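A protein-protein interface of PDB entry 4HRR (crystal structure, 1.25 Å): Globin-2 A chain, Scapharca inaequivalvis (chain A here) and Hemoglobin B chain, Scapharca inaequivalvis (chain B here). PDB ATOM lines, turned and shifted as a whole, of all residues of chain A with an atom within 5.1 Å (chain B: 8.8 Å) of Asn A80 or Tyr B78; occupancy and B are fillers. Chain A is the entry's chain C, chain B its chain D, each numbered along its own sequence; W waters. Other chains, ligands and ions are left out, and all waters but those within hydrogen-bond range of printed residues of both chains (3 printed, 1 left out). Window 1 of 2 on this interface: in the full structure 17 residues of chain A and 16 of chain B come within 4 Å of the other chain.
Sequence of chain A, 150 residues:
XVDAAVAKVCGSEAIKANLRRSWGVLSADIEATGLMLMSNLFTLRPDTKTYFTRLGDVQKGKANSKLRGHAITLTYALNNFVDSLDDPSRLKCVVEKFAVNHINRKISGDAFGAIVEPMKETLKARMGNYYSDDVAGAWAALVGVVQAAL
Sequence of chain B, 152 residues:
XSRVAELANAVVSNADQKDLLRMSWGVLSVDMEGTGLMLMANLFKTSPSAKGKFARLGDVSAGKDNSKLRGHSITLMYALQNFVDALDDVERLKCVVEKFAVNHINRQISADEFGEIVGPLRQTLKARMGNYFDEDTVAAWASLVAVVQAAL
The side-chain carboxylate (OD2) of Asp B85 is in hydrogen-bond range of the side-chain hydroxyl (OH) of Tyr A76 (2.5 Å).
The guanidinium group of Arg A90 sits at hydrogen-bond distance from the side-chain hydroxyl of Tyr B78 (3.1 Å).
OH of Tyr B78 is in hydrogen-bond range of OD2 of Asp A83 (2.5 Å).
The side-chain hydroxyl of Thr B75 sits at hydrogen-bond distance from the backbone carbonyl oxygen of Gly B71, 3.2 Å away.
The side-chain amide oxygen (OD1) of Asn A80 sits at hydrogen-bond distance from the guanidinium group (NH2) of Arg A90 (2.9 Å).
The guanidinium group (NH2) of Arg B70 is in salt-bridge range of the side-chain carboxylate (OE2) of Glu B33 (2.8 Å).
The side-chain carboxylate (OD1) of Asp B85 is in hydrogen-bond range of the side-chain amide nitrogen (NE2) of Gln B81, 3.2 Å away.
The indole nitrogen (NE1) of Trp B25 sits at hydrogen-bond distance from the side-chain amide oxygen (OE1) of Gln B81 (2.8 Å).
The side-chain carboxylate (OD2) of Asp A83 sits at hydrogen-bond distance from the side-chain amide nitrogen (ND2) of Asn A79 (3.2 Å).
Among the printed residues, pairs that only touch across the chains: Asn A80 with Ile B74 (3.4 Å), Tyr A76 with Asn B82 (3.5 Å), Arg A90 with Ile B74 (3.6 Å), Asn A80 with Tyr B78 (3.6 Å), Asn A80 with Thr B75 (3.7 Å), Arg A90 with Arg B70 (3.8 Å), Asn A79 with Tyr B78 (3.8 Å), Tyr A76 with Gln B81 (3.8 Å), Arg A90 with Glu B33 (3.9 Å) and Phe A98 with Thr B75 (3.9 Å).
Printed residues of chain B within 4 Å of Tyr A76: Gln B81 (3.8 Å), Asn B82 (3.5 Å) and Asp B85 (2.5 Å).
Ala A77 touches none of the printed residues of chain B.
Of chain B, only Ile B74, Thr B75 and Tyr B78 come within 4 Å of Asn A80.
Of chain B, only Tyr B78 (2.5 Å) comes within 4 Å of Asp A83.
Met B32 touches none of the printed residues of chain A.
Of the printed residues of chain A, Glu B33 touches Arg A90.
Printed residues of chain A within 4 Å of Tyr B78: Asn A79, Asn A80, Asp A83 and Arg A90.
Printed residues of chain A within 4 Å of Asn B82: Tyr A76 (3.5 Å).
Printed residues of chain A within 4 Å of Asp B85: Tyr A76 (2.5 Å).
The nearest printed residue of chain A that does not touch Tyr B78 is Tyr A76 (4.02 Å).
Among the printed residues, 13 pairs touch across the chains.
Among the printed residues, no Asp or Glu carboxylate lies within 4 Å of a Lys or Arg side-chain nitrogen of the other chain.
Water W3 lies within hydrogen-bond range of the backbone carbonyl oxygen (O) of Val A94 (2.6 Å) and the side-chain hydroxyl (OG1) of Thr B75 (3.4 Å).
Water W2 lies within hydrogen-bond range of OH of Tyr B78 (2.7 Å) and NH1 of Arg A90 (2.9 Å).
Water W1 bridges NH1 of Arg A90 and OE1 of Glu B33.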
ATOM      1  N   TYR A  76      -6.196  -6.508  11.947  1.00  0.00           N
ATOM      2  CA  TYR A  76      -7.454  -7.086  11.463  1.00  0.00           C
ATOM      3  C   TYR A  76      -8.497  -6.036  11.064  1.00  0.00           C
ATOM      4  O   TYR A  76      -9.337  -6.321  10.236  1.00  0.00           O
ATOM      5  CB  TYR A  76      -8.026  -8.109  12.458  1.00  0.00           C
ATOM      6  CG  TYR A  76      -7.207  -9.383  12.525  1.00  0.00           C
ATOM      7  CD1 TYR A  76      -7.093 -10.228  11.432  1.00  0.00           C
ATOM      8  CD2 TYR A  76      -6.530  -9.727  13.680  1.00  0.00           C
ATOM      9  CE1 TYR A  76      -6.324 -11.385  11.493  1.00  0.00           C
ATOM     10  CE2 TYR A  76      -5.764 -10.872  13.751  1.00  0.00           C
ATOM     11  CZ  TYR A  76      -5.655 -11.689  12.658  1.00  0.00           C
ATOM     12  OH  TYR A  76      -4.880 -12.814  12.752  1.00  0.00           O
ATOM     13  N   ALA A  77      -8.436  -4.844  11.648  1.00  0.00           N
ATOM     14  CA  ALA A  77      -9.264  -3.743  11.196  1.00  0.00           C
ATOM     15  C   ALA A  77      -8.887  -3.357   9.773  1.00  0.00           C
ATOM     16  O   ALA A  77      -9.772  -3.101   8.953  1.00  0.00           O
ATOM     17  CB  ALA A  77      -9.180  -2.549  12.138  1.00  0.00           C
ATOM     18  N   LEU A  78      -7.595  -3.320   9.473  1.00  0.00           N
ATOM     19  CA  LEU A  78      -7.132  -3.073   8.105  1.00  0.00           C
ATOM     20  C   LEU A  78      -7.615  -4.166   7.164  1.00  0.00           C
ATOM     21  O   LEU A  78      -8.053  -3.887   6.051  1.00  0.00           O
ATOM     22  CB  LEU A  78      -5.606  -2.957   8.033  1.00  0.00           C
ATOM     23  CG  LEU A  78      -5.001  -1.893   8.942  1.00  0.00           C
ATOM     24  CD1 LEU A  78      -3.492  -1.943   8.766  1.00  0.00           C
ATOM     25  CD2 LEU A  78      -5.536  -0.482   8.701  1.00  0.00           C
ATOM     26  N   ASN A  79      -7.542  -5.413   7.618  1.00  0.00           N
ATOM     27  CA  ASN A  79      -8.005  -6.579   6.845  1.00  0.00           C
ATOM     28  C   ASN A  79      -9.483  -6.404   6.497  1.00  0.00           C
ATOM     29  O   ASN A  79      -9.906  -6.611   5.356  1.00  0.00           O
ATOM     30  CB  ASN A  79      -7.808  -7.837   7.710  1.00  0.00           C
ATOM     31  CG  ASN A  79      -7.924  -9.165   6.971  1.00  0.00           C
ATOM     32  OD1 ASN A  79      -7.579 -10.179   7.573  1.00  0.00           O
ATOM     33  ND2 ASN A  79      -8.394  -9.191   5.715  1.00  0.00           N
ATOM     34  N   ASN A  80     -10.259  -5.983   7.489  1.00  0.00           N
ATOM     35  CA  ASN A  80     -11.695  -5.706   7.359  1.00  0.00           C
ATOM     36  C   ASN A  80     -11.937  -4.622   6.311  1.00  0.00           C
ATOM     37  O   ASN A  80     -12.775  -4.789   5.427  1.00  0.00           O
ATOM     38  CB  ASN A  80     -12.197  -5.314   8.755  1.00  0.00           C
ATOM     39  CG  ASN A  80     -13.707  -5.258   8.872  1.00  0.00           C
ATOM     40  OD1 ASN A  80     -14.448  -5.276   7.878  1.00  0.00           O
ATOM     41  ND2 ASN A  80     -14.178  -5.173  10.125  1.00  0.00           N
ATOM     42  N   PHE A  81     -11.207  -3.515   6.381  1.00  0.00           N
ATOM     43  CA  PHE A  81     -11.352  -2.478   5.363  1.00  0.00           C
ATOM     44  C   PHE A  81     -11.142  -3.042   3.954  1.00  0.00           C
ATOM     45  O   PHE A  81     -11.914  -2.762   3.030  1.00  0.00           O
ATOM     46  CB  PHE A  81     -10.371  -1.329   5.576  1.00  0.00           C
ATOM     47  CG  PHE A  81     -10.658  -0.462   6.779  1.00  0.00           C
ATOM     48  CD1 PHE A  81     -11.932  -0.331   7.307  1.00  0.00           C
ATOM     49  CD2 PHE A  81      -9.640   0.239   7.371  1.00  0.00           C
ATOM     50  CE1 PHE A  81     -12.177   0.474   8.412  1.00  0.00           C
ATOM     51  CE2 PHE A  81      -9.890   1.068   8.464  1.00  0.00           C
ATOM     52  CZ  PHE A  81     -11.161   1.174   8.987  1.00  0.00           C
ATOM     53  N   VAL A  82     -10.075  -3.823   3.791  1.00  0.00           N
ATOM     54  CA  VAL A  82      -9.724  -4.361   2.482  1.00  0.00           C
ATOM     55  C   VAL A  82     -10.828  -5.291   1.976  1.00  0.00           C
ATOM     56  O   VAL A  82     -11.130  -5.297   0.786  1.00  0.00           O
ATOM     57  CB  VAL A  82      -8.355  -5.077   2.516  1.00  0.00           C
ATOM     58  CG1 VAL A  82      -8.083  -5.774   1.200  1.00  0.00           C
ATOM     59  CG2 VAL A  82      -7.263  -4.062   2.822  1.00  0.00           C
ATOM     60  N   ASP A  83     -11.451  -6.043   2.875  1.00  0.00           N
ATOM     61  CA  ASP A  83     -12.562  -6.935   2.526  1.00  0.00           C
ATOM     62  C   ASP A  83     -13.917  -6.213   2.394  1.00  0.00           C
ATOM     63  O   ASP A  83     -14.925  -6.861   2.102  1.00  0.00           O
ATOM     64  CB  ASP A  83     -12.679  -8.061   3.551  1.00  0.00           C
ATOM     65  CG  ASP A  83     -11.531  -9.038   3.502  1.00  0.00           C
ATOM     66  OD1 ASP A  83     -10.848  -9.144   2.465  1.00  0.00           O
ATOM     67  OD2 ASP A  83     -11.338  -9.723   4.521  1.00  0.00           O
ATOM     68  N   SER A  84     -13.933  -4.892   2.599  1.00  0.00           N
ATOM     69  CA  SER A  84     -15.145  -4.070   2.521  1.00  0.00           C
ATOM     70  C   SER A  84     -15.240  -3.296   1.206  1.00  0.00           C
ATOM     71  O   SER A  84     -16.174  -2.507   1.028  1.00  0.00           O
ATOM     72  CB  SER A  84     -15.171  -3.059   3.678  1.00  0.00           C
ATOM     73  OG  SER A  84     -15.195  -3.689   4.938  1.00  0.00           O
ATOM     74  N   ARG A  90     -20.987  -1.574   3.190  1.00  0.00           N
ATOM     75  CA  ARG A  90     -20.181  -2.314   4.167  1.00  0.00           C
ATOM     76  C   ARG A  90     -19.058  -1.415   4.662  1.00  0.00           C
ATOM     77  O   ARG A  90     -18.857  -1.261   5.863  1.00  0.00           O
ATOM     78  CB  ARG A  90     -19.601  -3.621   3.621  1.00  0.00           C
ATOM     79  CG  ARG A  90     -18.681  -4.261   4.646  1.00  0.00           C
ATOM     80  CD  ARG A  90     -18.205  -5.662   4.316  1.00  0.00           C
ATOM     81  NE  ARG A  90     -16.941  -5.918   5.010  1.00  0.00           N
ATOM     82  CZ  ARG A  90     -16.350  -7.104   5.152  1.00  0.00           C
ATOM     83  NH1 ARG A  90     -16.906  -8.213   4.675  1.00  0.00           N
ATOM     84  NH2 ARG A  90     -15.181  -7.162   5.793  1.00  0.00           N
ATOM     85  N   VAL A  94     -18.573  -0.272   8.606  1.00  0.00           N
ATOM     86  CA  VAL A  94     -17.343  -0.704   9.269  1.00  0.00           C
ATOM     87  C   VAL A  94     -16.561   0.524   9.741  1.00  0.00           C
ATOM     88  O   VAL A  94     -16.100   0.588  10.875  1.00  0.00           O
ATOM     89  CB  VAL A  94     -16.524  -1.615   8.329  1.00  0.00           C
ATOM     90  CG1 VAL A  94     -15.100  -1.801   8.830  1.00  0.00           C
ATOM     91  CG2 VAL A  94     -17.201  -2.972   8.189  1.00  0.00           C
ATOM     92  N   PHE A  98     -15.691   1.725  13.707  1.00  0.00           N
ATOM     93  CA  PHE A  98     -14.377   2.107  14.215  1.00  0.00           C
ATOM     94  C   PHE A  98     -14.334   3.589  14.639  1.00  0.00           C
ATOM     95  O   PHE A  98     -13.617   3.939  15.589  1.00  0.00           O
ATOM     96  CB  PHE A  98     -13.230   1.686  13.258  1.00  0.00           C
ATOM     97  CG  PHE A  98     -13.018   0.186  13.197  1.00  0.00           C
ATOM     98  CD1 PHE A  98     -12.804  -0.550  14.361  1.00  0.00           C
ATOM     99  CD2 PHE A  98     -13.071  -0.499  11.987  1.00  0.00           C
ATOM    100  CE1 PHE A  98     -12.630  -1.929  14.323  1.00  0.00           C
ATOM    101  CE2 PHE A  98     -12.891  -1.879  11.940  1.00  0.00           C
ATOM    102  CZ  PHE A  98     -12.682  -2.594  13.109  1.00  0.00           C
ATOM    103  N   TRP B  25     -13.261 -23.202  10.200  1.00  0.00           N
ATOM    104  CA  TRP B  25     -12.988 -21.826   9.780  1.00  0.00           C
ATOM    105  C   TRP B  25     -13.046 -21.671   8.256  1.00  0.00           C
ATOM    106  O   TRP B  25     -13.506 -20.656   7.735  1.00  0.00           O
ATOM    107  CB  TRP B  25     -11.638 -21.316  10.329  1.00  0.00           C
ATOM    108  CG  TRP B  25     -11.433 -19.869  10.003  1.00  0.00           C
ATOM    109  CD1 TRP B  25     -10.501 -19.330   9.172  1.00  0.00           C
ATOM    110  CD2 TRP B  25     -12.246 -18.782  10.450  1.00  0.00           C
ATOM    111  NE1 TRP B  25     -10.675 -17.967   9.074  1.00  0.00           N
ATOM    112  CE2 TRP B  25     -11.723 -17.611   9.878  1.00  0.00           C
ATOM    113  CE3 TRP B  25     -13.348 -18.683  11.314  1.00  0.00           C
ATOM    114  CZ2 TRP B  25     -12.291 -16.366  10.099  1.00  0.00           C
ATOM    115  CZ3 TRP B  25     -13.910 -17.434  11.533  1.00  0.00           C
ATOM    116  CH2 TRP B  25     -13.378 -16.297  10.933  1.00  0.00           C
ATOM    117  N   SER B  29     -15.684 -18.711   7.177  1.00  0.00           N
ATOM    118  CA  SER B  29     -15.094 -17.482   6.643  1.00  0.00           C
ATOM    119  C   SER B  29     -15.356 -17.244   5.145  1.00  0.00           C
ATOM    120  O   SER B  29     -14.930 -16.229   4.603  1.00  0.00           O
ATOM    121  CB  SER B  29     -13.591 -17.460   6.939  1.00  0.00           C
ATOM    122  OG  SER B  29     -12.934 -18.454   6.210  1.00  0.00           O
ATOM    123  N   ASP B  31     -18.170 -16.421   3.866  1.00  0.00           N
ATOM    124  CA  ASP B  31     -19.057 -15.258   3.873  1.00  0.00           C
ATOM    125  C   ASP B  31     -19.007 -14.692   5.284  1.00  0.00           C
ATOM    126  O   ASP B  31     -19.872 -14.957   6.111  1.00  0.00           O
ATOM    127  CB  ASP B  31     -20.469 -15.697   3.498  1.00  0.00           C
ATOM    128  CG  ASP B  31     -21.507 -14.570   3.568  1.00  0.00           C
ATOM    129  OD1 ASP B  31     -21.138 -13.375   3.687  1.00  0.00           O
ATOM    130  OD2 ASP B  31     -22.704 -14.933   3.544  1.00  0.00           O
ATOM    131  N   MET B  32     -17.970 -13.916   5.562  1.00  0.00           N
ATOM    132  CA  MET B  32     -17.739 -13.390   6.900  1.00  0.00           C
ATOM    133  C   MET B  32     -18.950 -12.598   7.393  1.00  0.00           C
ATOM    134  O   MET B  32     -19.408 -12.755   8.522  1.00  0.00           O
ATOM    135  CB  MET B  32     -16.510 -12.478   6.907  1.00  0.00           C
ATOM    136  CG  MET B  32     -15.189 -13.188   6.641  1.00  0.00           C
ATOM    137  SD  MET B  32     -14.598 -14.077   8.092  1.00  0.00           S
ATOM    138  CE  MET B  32     -13.694 -12.792   8.959  1.00  0.00           C
ATOM    139  N   GLU B  33     -19.461 -11.716   6.540  1.00  0.00           N
ATOM    140  CA  GLU B  33     -20.584 -10.881   6.932  1.00  0.00           C
ATOM    141  C   GLU B  33     -21.832 -11.716   7.246  1.00  0.00           C
ATOM    142  O   GLU B  33     -22.469 -11.548   8.294  1.00  0.00           O
ATOM    143  CB  GLU B  33     -20.865  -9.858   5.832  1.00  0.00           C
ATOM    144  CG  GLU B  33     -22.059  -8.968   6.094  1.00  0.00           C
ATOM    145  CD  GLU B  33     -22.315  -7.946   5.001  1.00  0.00           C
ATOM    146  OE1 GLU B  33     -21.450  -7.761   4.107  1.00  0.00           O
ATOM    147  OE2 GLU B  33     -23.402  -7.341   5.014  1.00  0.00           O
ATOM    148  N   GLY B  36     -21.305 -13.866  10.357  1.00  0.00           N
ATOM    149  CA  GLY B  36     -21.352 -13.037  11.563  1.00  0.00           C
ATOM    150  C   GLY B  36     -22.787 -12.704  11.953  1.00  0.00           C
ATOM    151  O   GLY B  36     -23.162 -12.784  13.106  1.00  0.00           O
ATOM    152  N   ARG B  70     -24.604  -4.849  11.371  1.00  0.00           N
ATOM    153  CA  ARG B  70     -23.668  -5.354  10.350  1.00  0.00           C
ATOM    154  C   ARG B  70     -22.221  -5.058  10.717  1.00  0.00           C
ATOM    155  O   ARG B  70     -21.378  -5.940  10.647  1.00  0.00           O
ATOM    156  CB  ARG B  70     -23.890  -4.730   8.980  1.00  0.00           C
ATOM    157  CG  ARG B  70     -25.167  -5.054   8.224  1.00  0.00           C
ATOM    158  CD  ARG B  70     -25.164  -4.256   6.929  1.00  0.00           C
ATOM    159  NE  ARG B  70     -24.274  -4.799   5.903  1.00  0.00           N
ATOM    160  CZ  ARG B  70     -23.933  -4.162   4.785  1.00  0.00           C
ATOM    161  NH1 ARG B  70     -24.351  -2.924   4.547  1.00  0.00           N
ATOM    162  NH2 ARG B  70     -23.177  -4.761   3.883  1.00  0.00           N
ATOM    163  N   GLY B  71     -21.925  -3.830  11.118  1.00  0.00           N
ATOM    164  CA  GLY B  71     -20.558  -3.458  11.471  1.00  0.00           C
ATOM    165  C   GLY B  71     -20.031  -4.311  12.610  1.00  0.00           C
ATOM    166  O   GLY B  71     -18.905  -4.803  12.578  1.00  0.00           O
ATOM    167  N   HIS B  72     -20.848  -4.488  13.635  1.00  0.00           N
ATOM    168  CA  HIS B  72     -20.474  -5.313  14.759  1.00  0.00           C
ATOM    169  C   HIS B  72     -20.221  -6.767  14.356  1.00  0.00           C
ATOM    170  O   HIS B  72     -19.224  -7.377  14.757  1.00  0.00           O
ATOM    171  CB  HIS B  72     -21.532  -5.280  15.857  1.00  0.00           C
ATOM    172  CG  HIS B  72     -21.307  -6.334  16.860  1.00  0.00           C
ATOM    173  ND1 HIS B  72     -20.282  -6.243  17.773  1.00  0.00           N
ATOM    174  CD2 HIS B  72     -21.851  -7.559  16.997  1.00  0.00           C
ATOM    175  CE1 HIS B  72     -20.233  -7.364  18.466  1.00  0.00           C
ATOM    176  NE2 HIS B  72     -21.175  -8.176  18.016  1.00  0.00           N
ATOM    177  N   SER B  73     -21.162  -7.333  13.608  1.00  0.00           N
ATOM    178  CA  SER B  73     -21.127  -8.743  13.249  1.00  0.00           C
ATOM    179  C   SER B  73     -19.928  -9.081  12.402  1.00  0.00           C
ATOM    180  O   SER B  73     -19.325 -10.135  12.575  1.00  0.00           O
ATOM    181  CB  SER B  73     -22.386  -9.138  12.492  1.00  0.00           C
ATOM    182  OG  SER B  73     -23.555  -8.990  13.272  1.00  0.00           O
ATOM    183  N   ILE B  74     -19.570  -8.187  11.495  1.00  0.00           N
ATOM    184  CA  ILE B  74     -18.348  -8.362  10.711  1.00  0.00           C
ATOM    185  C   ILE B  74     -17.092  -8.354  11.596  1.00  0.00           C
ATOM    186  O   ILE B  74     -16.190  -9.214  11.448  1.00  0.00           O
ATOM    187  CB  ILE B  74     -18.253  -7.286   9.611  1.00  0.00           C
ATOM    188  CG1 ILE B  74     -19.389  -7.472   8.594  1.00  0.00           C
ATOM    189  CG2 ILE B  74     -16.911  -7.336   8.890  1.00  0.00           C
ATOM    190  CD1 ILE B  74     -19.640  -6.267   7.714  1.00  0.00           C
ATOM    191  N   THR B  75     -17.023  -7.405  12.527  1.00  0.00           N
ATOM    192  CA  THR B  75     -15.862  -7.303  13.408  1.00  0.00           C
ATOM    193  C   THR B  75     -15.739  -8.559  14.281  1.00  0.00           C
ATOM    194  O   THR B  75     -14.623  -9.036  14.574  1.00  0.00           O
ATOM    195  CB  THR B  75     -15.930  -6.018  14.250  1.00  0.00           C
ATOM    196  OG1 THR B  75     -15.816  -4.897  13.377  1.00  0.00           O
ATOM    197  CG2 THR B  75     -14.801  -5.972  15.266  1.00  0.00           C
ATOM    198  N   LEU B  76     -16.877  -9.088  14.720  1.00  0.00           N
ATOM    199  CA  LEU B  76     -16.863 -10.331  15.501  1.00  0.00           C
ATOM    200  C   LEU B  76     -16.164 -11.458  14.736  1.00  0.00           C
ATOM    201  O   LEU B  76     -15.374 -12.221  15.300  1.00  0.00           O
ATOM    202  CB  LEU B  76     -18.292 -10.735  15.886  1.00  0.00           C
ATOM    203  CG  LEU B  76     -18.464 -12.104  16.569  1.00  0.00           C
ATOM    204  CD1 LEU B  76     -17.701 -12.229  17.888  1.00  0.00           C
ATOM    205  CD2 LEU B  76     -19.961 -12.319  16.799  1.00  0.00           C
ATOM    206  N   MET B  77     -16.450 -11.558  13.445  1.00  0.00           N
ATOM    207  CA  MET B  77     -15.797 -12.572  12.631  1.00  0.00           C
ATOM    208  C   MET B  77     -14.297 -12.374  12.497  1.00  0.00           C
ATOM    209  O   MET B  77     -13.568 -13.360  12.506  1.00  0.00           O
ATOM    210  CB  MET B  77     -16.476 -12.680  11.272  1.00  0.00           C
ATOM    211  CG  MET B  77     -17.905 -13.189  11.381  1.00  0.00           C
ATOM    212  SD  MET B  77     -18.078 -14.837  12.064  1.00  0.00           S
ATOM    213  CE  MET B  77     -17.332 -15.772  10.739  1.00  0.00           C
ATOM    214  N   TYR B  78     -13.804 -11.150  12.409  1.00  0.00           N
ATOM    215  CA  TYR B  78     -12.342 -10.946  12.477  1.00  0.00           C
ATOM    216  C   TYR B  78     -11.743 -11.295  13.832  1.00  0.00           C
ATOM    217  O   TYR B  78     -10.582 -11.656  13.895  1.00  0.00           O
ATOM    218  CB  TYR B  78     -11.953  -9.539  12.013  1.00  0.00           C
ATOM    219  CG  TYR B  78     -12.157  -9.394  10.531  1.00  0.00           C
ATOM    220  CD1 TYR B  78     -11.196  -9.825   9.613  1.00  0.00           C
ATOM    221  CD2 TYR B  78     -13.366  -8.905  10.030  1.00  0.00           C
ATOM    222  CE1 TYR B  78     -11.421  -9.751   8.251  1.00  0.00           C
ATOM    223  CE2 TYR B  78     -13.596  -8.821   8.680  1.00  0.00           C
ATOM    224  CZ  TYR B  78     -12.619  -9.228   7.800  1.00  0.00           C
ATOM    225  OH  TYR B  78     -12.879  -9.136   6.459  1.00  0.00           O
ATOM    226  N   ALA B  79     -12.522 -11.216  14.902  1.00  0.00           N
ATOM    227  CA  ALA B  79     -12.061 -11.667  16.202  1.00  0.00           C
ATOM    228  C   ALA B  79     -11.903 -13.179  16.184  1.00  0.00           C
ATOM    229  O   ALA B  79     -10.934 -13.703  16.747  1.00  0.00           O
ATOM    230  CB  ALA B  79     -13.011 -11.214  17.300  1.00  0.00           C
ATOM    231  N   LEU B  80     -12.779 -13.903  15.503  1.00  0.00           N
ATOM    232  CA  LEU B  80     -12.600 -15.347  15.365  1.00  0.00           C
ATOM    233  C   LEU B  80     -11.399 -15.656  14.471  1.00  0.00           C
ATOM    234  O   LEU B  80     -10.625 -16.577  14.765  1.00  0.00           O
ATOM    235  CB  LEU B  80     -13.874 -16.009  14.840  1.00  0.00           C
ATOM    236  CG  LEU B  80     -15.126 -15.880  15.713  1.00  0.00           C
ATOM    237  CD1 LEU B  80     -16.275 -16.679  15.085  1.00  0.00           C
ATOM    238  CD2 LEU B  80     -14.878 -16.310  17.143  1.00  0.00           C
ATOM    239  N   GLN B  81     -11.186 -14.880  13.417  1.00  0.00           N
ATOM    240  CA  GLN B  81      -9.959 -15.042  12.594  1.00  0.00           C
ATOM    241  C   GLN B  81      -8.715 -14.853  13.441  1.00  0.00           C
ATOM    242  O   GLN B  81      -7.742 -15.595  13.297  1.00  0.00           O
ATOM    243  CB  GLN B  81      -9.970 -14.034  11.442  1.00  0.00           C
ATOM    244  CG  GLN B  81      -8.766 -14.127  10.513  1.00  0.00           C
ATOM    245  CD  GLN B  81      -8.774 -15.367   9.650  1.00  0.00           C
ATOM    246  OE1 GLN B  81      -9.550 -15.474   8.708  1.00  0.00           O
ATOM    247  NE2 GLN B  81      -7.915 -16.307   9.965  1.00  0.00           N
ATOM    248  N   ASN B  82      -8.752 -13.835  14.298  1.00  0.00           N
ATOM    249  CA  ASN B  82      -7.670 -13.547  15.257  1.00  0.00           C
ATOM    250  C   ASN B  82      -7.333 -14.812  16.094  1.00  0.00           C
ATOM    251  O   ASN B  82      -6.182 -15.253  16.149  1.00  0.00           O
ATOM    252  CB  ASN B  82      -8.146 -12.359  16.105  1.00  0.00           C
ATOM    253  CG  ASN B  82      -7.058 -11.657  16.877  1.00  0.00           C
ATOM    254  OD1 ASN B  82      -6.002 -12.212  17.161  1.00  0.00           O
ATOM    255  ND2 ASN B  82      -7.335 -10.417  17.258  1.00  0.00           N
ATOM    256  N   PHE B  83      -8.340 -15.402  16.729  1.00  0.00           N
ATOM    257  CA  PHE B  83      -8.150 -16.680  17.438  1.00  0.00           C
ATOM    258  C   PHE B  83      -7.482 -17.718  16.543  1.00  0.00           C
ATOM    259  O   PHE B  83      -6.512 -18.357  16.945  1.00  0.00           O
ATOM    260  CB  PHE B  83      -9.496 -17.274  17.885  1.00  0.00           C
ATOM    261  CG  PHE B  83      -9.994 -16.838  19.233  1.00  0.00           C
ATOM    262  CD1 PHE B  83      -9.180 -16.855  20.348  1.00  0.00           C
ATOM    263  CD2 PHE B  83     -11.342 -16.535  19.392  1.00  0.00           C
ATOM    264  CE1 PHE B  83      -9.684 -16.513  21.591  1.00  0.00           C
ATOM    265  CE2 PHE B  83     -11.851 -16.197  20.637  1.00  0.00           C
ATOM    266  CZ  PHE B  83     -11.018 -16.179  21.733  1.00  0.00           C
ATOM    267  N   VAL B  84      -8.013 -17.916  15.340  1.00  0.00           N
ATOM    268  CA  VAL B  84      -7.522 -18.969  14.460  1.00  0.00           C
ATOM    269  C   VAL B  84      -6.054 -18.739  14.119  1.00  0.00           C
ATOM    270  O   VAL B  84      -5.301 -19.698  13.979  1.00  0.00           O
ATOM    271  CB  VAL B  84      -8.368 -19.054  13.181  1.00  0.00           C
ATOM    272  CG1 VAL B  84      -7.702 -19.920  12.122  1.00  0.00           C
ATOM    273  CG2 VAL B  84      -9.738 -19.591  13.524  1.00  0.00           C
ATOM    274  N   ASP B  85      -5.658 -17.479  13.988  1.00  0.00           N
ATOM    275  CA  ASP B  85      -4.274 -17.136  13.662  1.00  0.00           C
ATOM    276  C   ASP B  85      -3.314 -17.170  14.861  1.00  0.00           C
ATOM    277  O   ASP B  85      -2.103 -17.036  14.684  1.00  0.00           O
ATOM    278  CB  ASP B  85      -4.225 -15.767  12.986  1.00  0.00           C
ATOM    279  CG  ASP B  85      -4.788 -15.787  11.583  1.00  0.00           C
ATOM    280  OD1 ASP B  85      -4.960 -16.873  10.993  1.00  0.00           O
ATOM    281  OD2 ASP B  85      -5.041 -14.700  11.054  1.00  0.00           O
ATOM    282  N   VAL B  96      -4.220 -11.832  22.982  1.00  0.00           N
ATOM    283  CA  VAL B  96      -5.481 -11.678  22.255  1.00  0.00           C
ATOM    284  C   VAL B  96      -6.670 -11.897  23.195  1.00  0.00           C
ATOM    285  O   VAL B  96      -7.636 -11.122  23.214  1.00  0.00           O
ATOM    286  CB  VAL B  96      -5.508 -12.661  21.056  1.00  0.00           C
ATOM    287  CG1 VAL B  96      -6.915 -12.812  20.489  1.00  0.00           C
ATOM    288  CG2 VAL B  96      -4.522 -12.197  19.992  1.00  0.00           C
ATOM    289  N   PHE B 100      -9.618  -9.218  24.522  1.00  0.00           N
ATOM    290  CA  PHE B 100     -11.040  -9.552  24.501  1.00  0.00           C
ATOM    291  C   PHE B 100     -11.652  -9.429  25.883  1.00  0.00           C
ATOM    292  O   PHE B 100     -12.757  -8.920  26.023  1.00  0.00           O
ATOM    293  CB  PHE B 100     -11.304 -10.983  24.022  1.00  0.00           C
ATOM    294  CG  PHE B 100     -11.024 -11.226  22.565  1.00  0.00           C
ATOM    295  CD1 PHE B 100     -11.158 -10.226  21.605  1.00  0.00           C
ATOM    296  CD2 PHE B 100     -10.658 -12.498  22.148  1.00  0.00           C
ATOM    297  CE1 PHE B 100     -10.911 -10.508  20.265  1.00  0.00           C
ATOM    298  CE2 PHE B 100     -10.411 -12.780  20.818  1.00  0.00           C
ATOM    299  CZ  PHE B 100     -10.519 -11.782  19.876  1.00  0.00           C
HETATM  300  O   HOH W   1     -19.047  -8.767   2.950  1.00  0.00           O
HETATM  301  O   HOH W   2     -14.923 -10.284   5.024  1.00  0.00           O
HETATM  302  O   HOH W   3     -15.691  -1.664  12.199  1.00  0.00           O
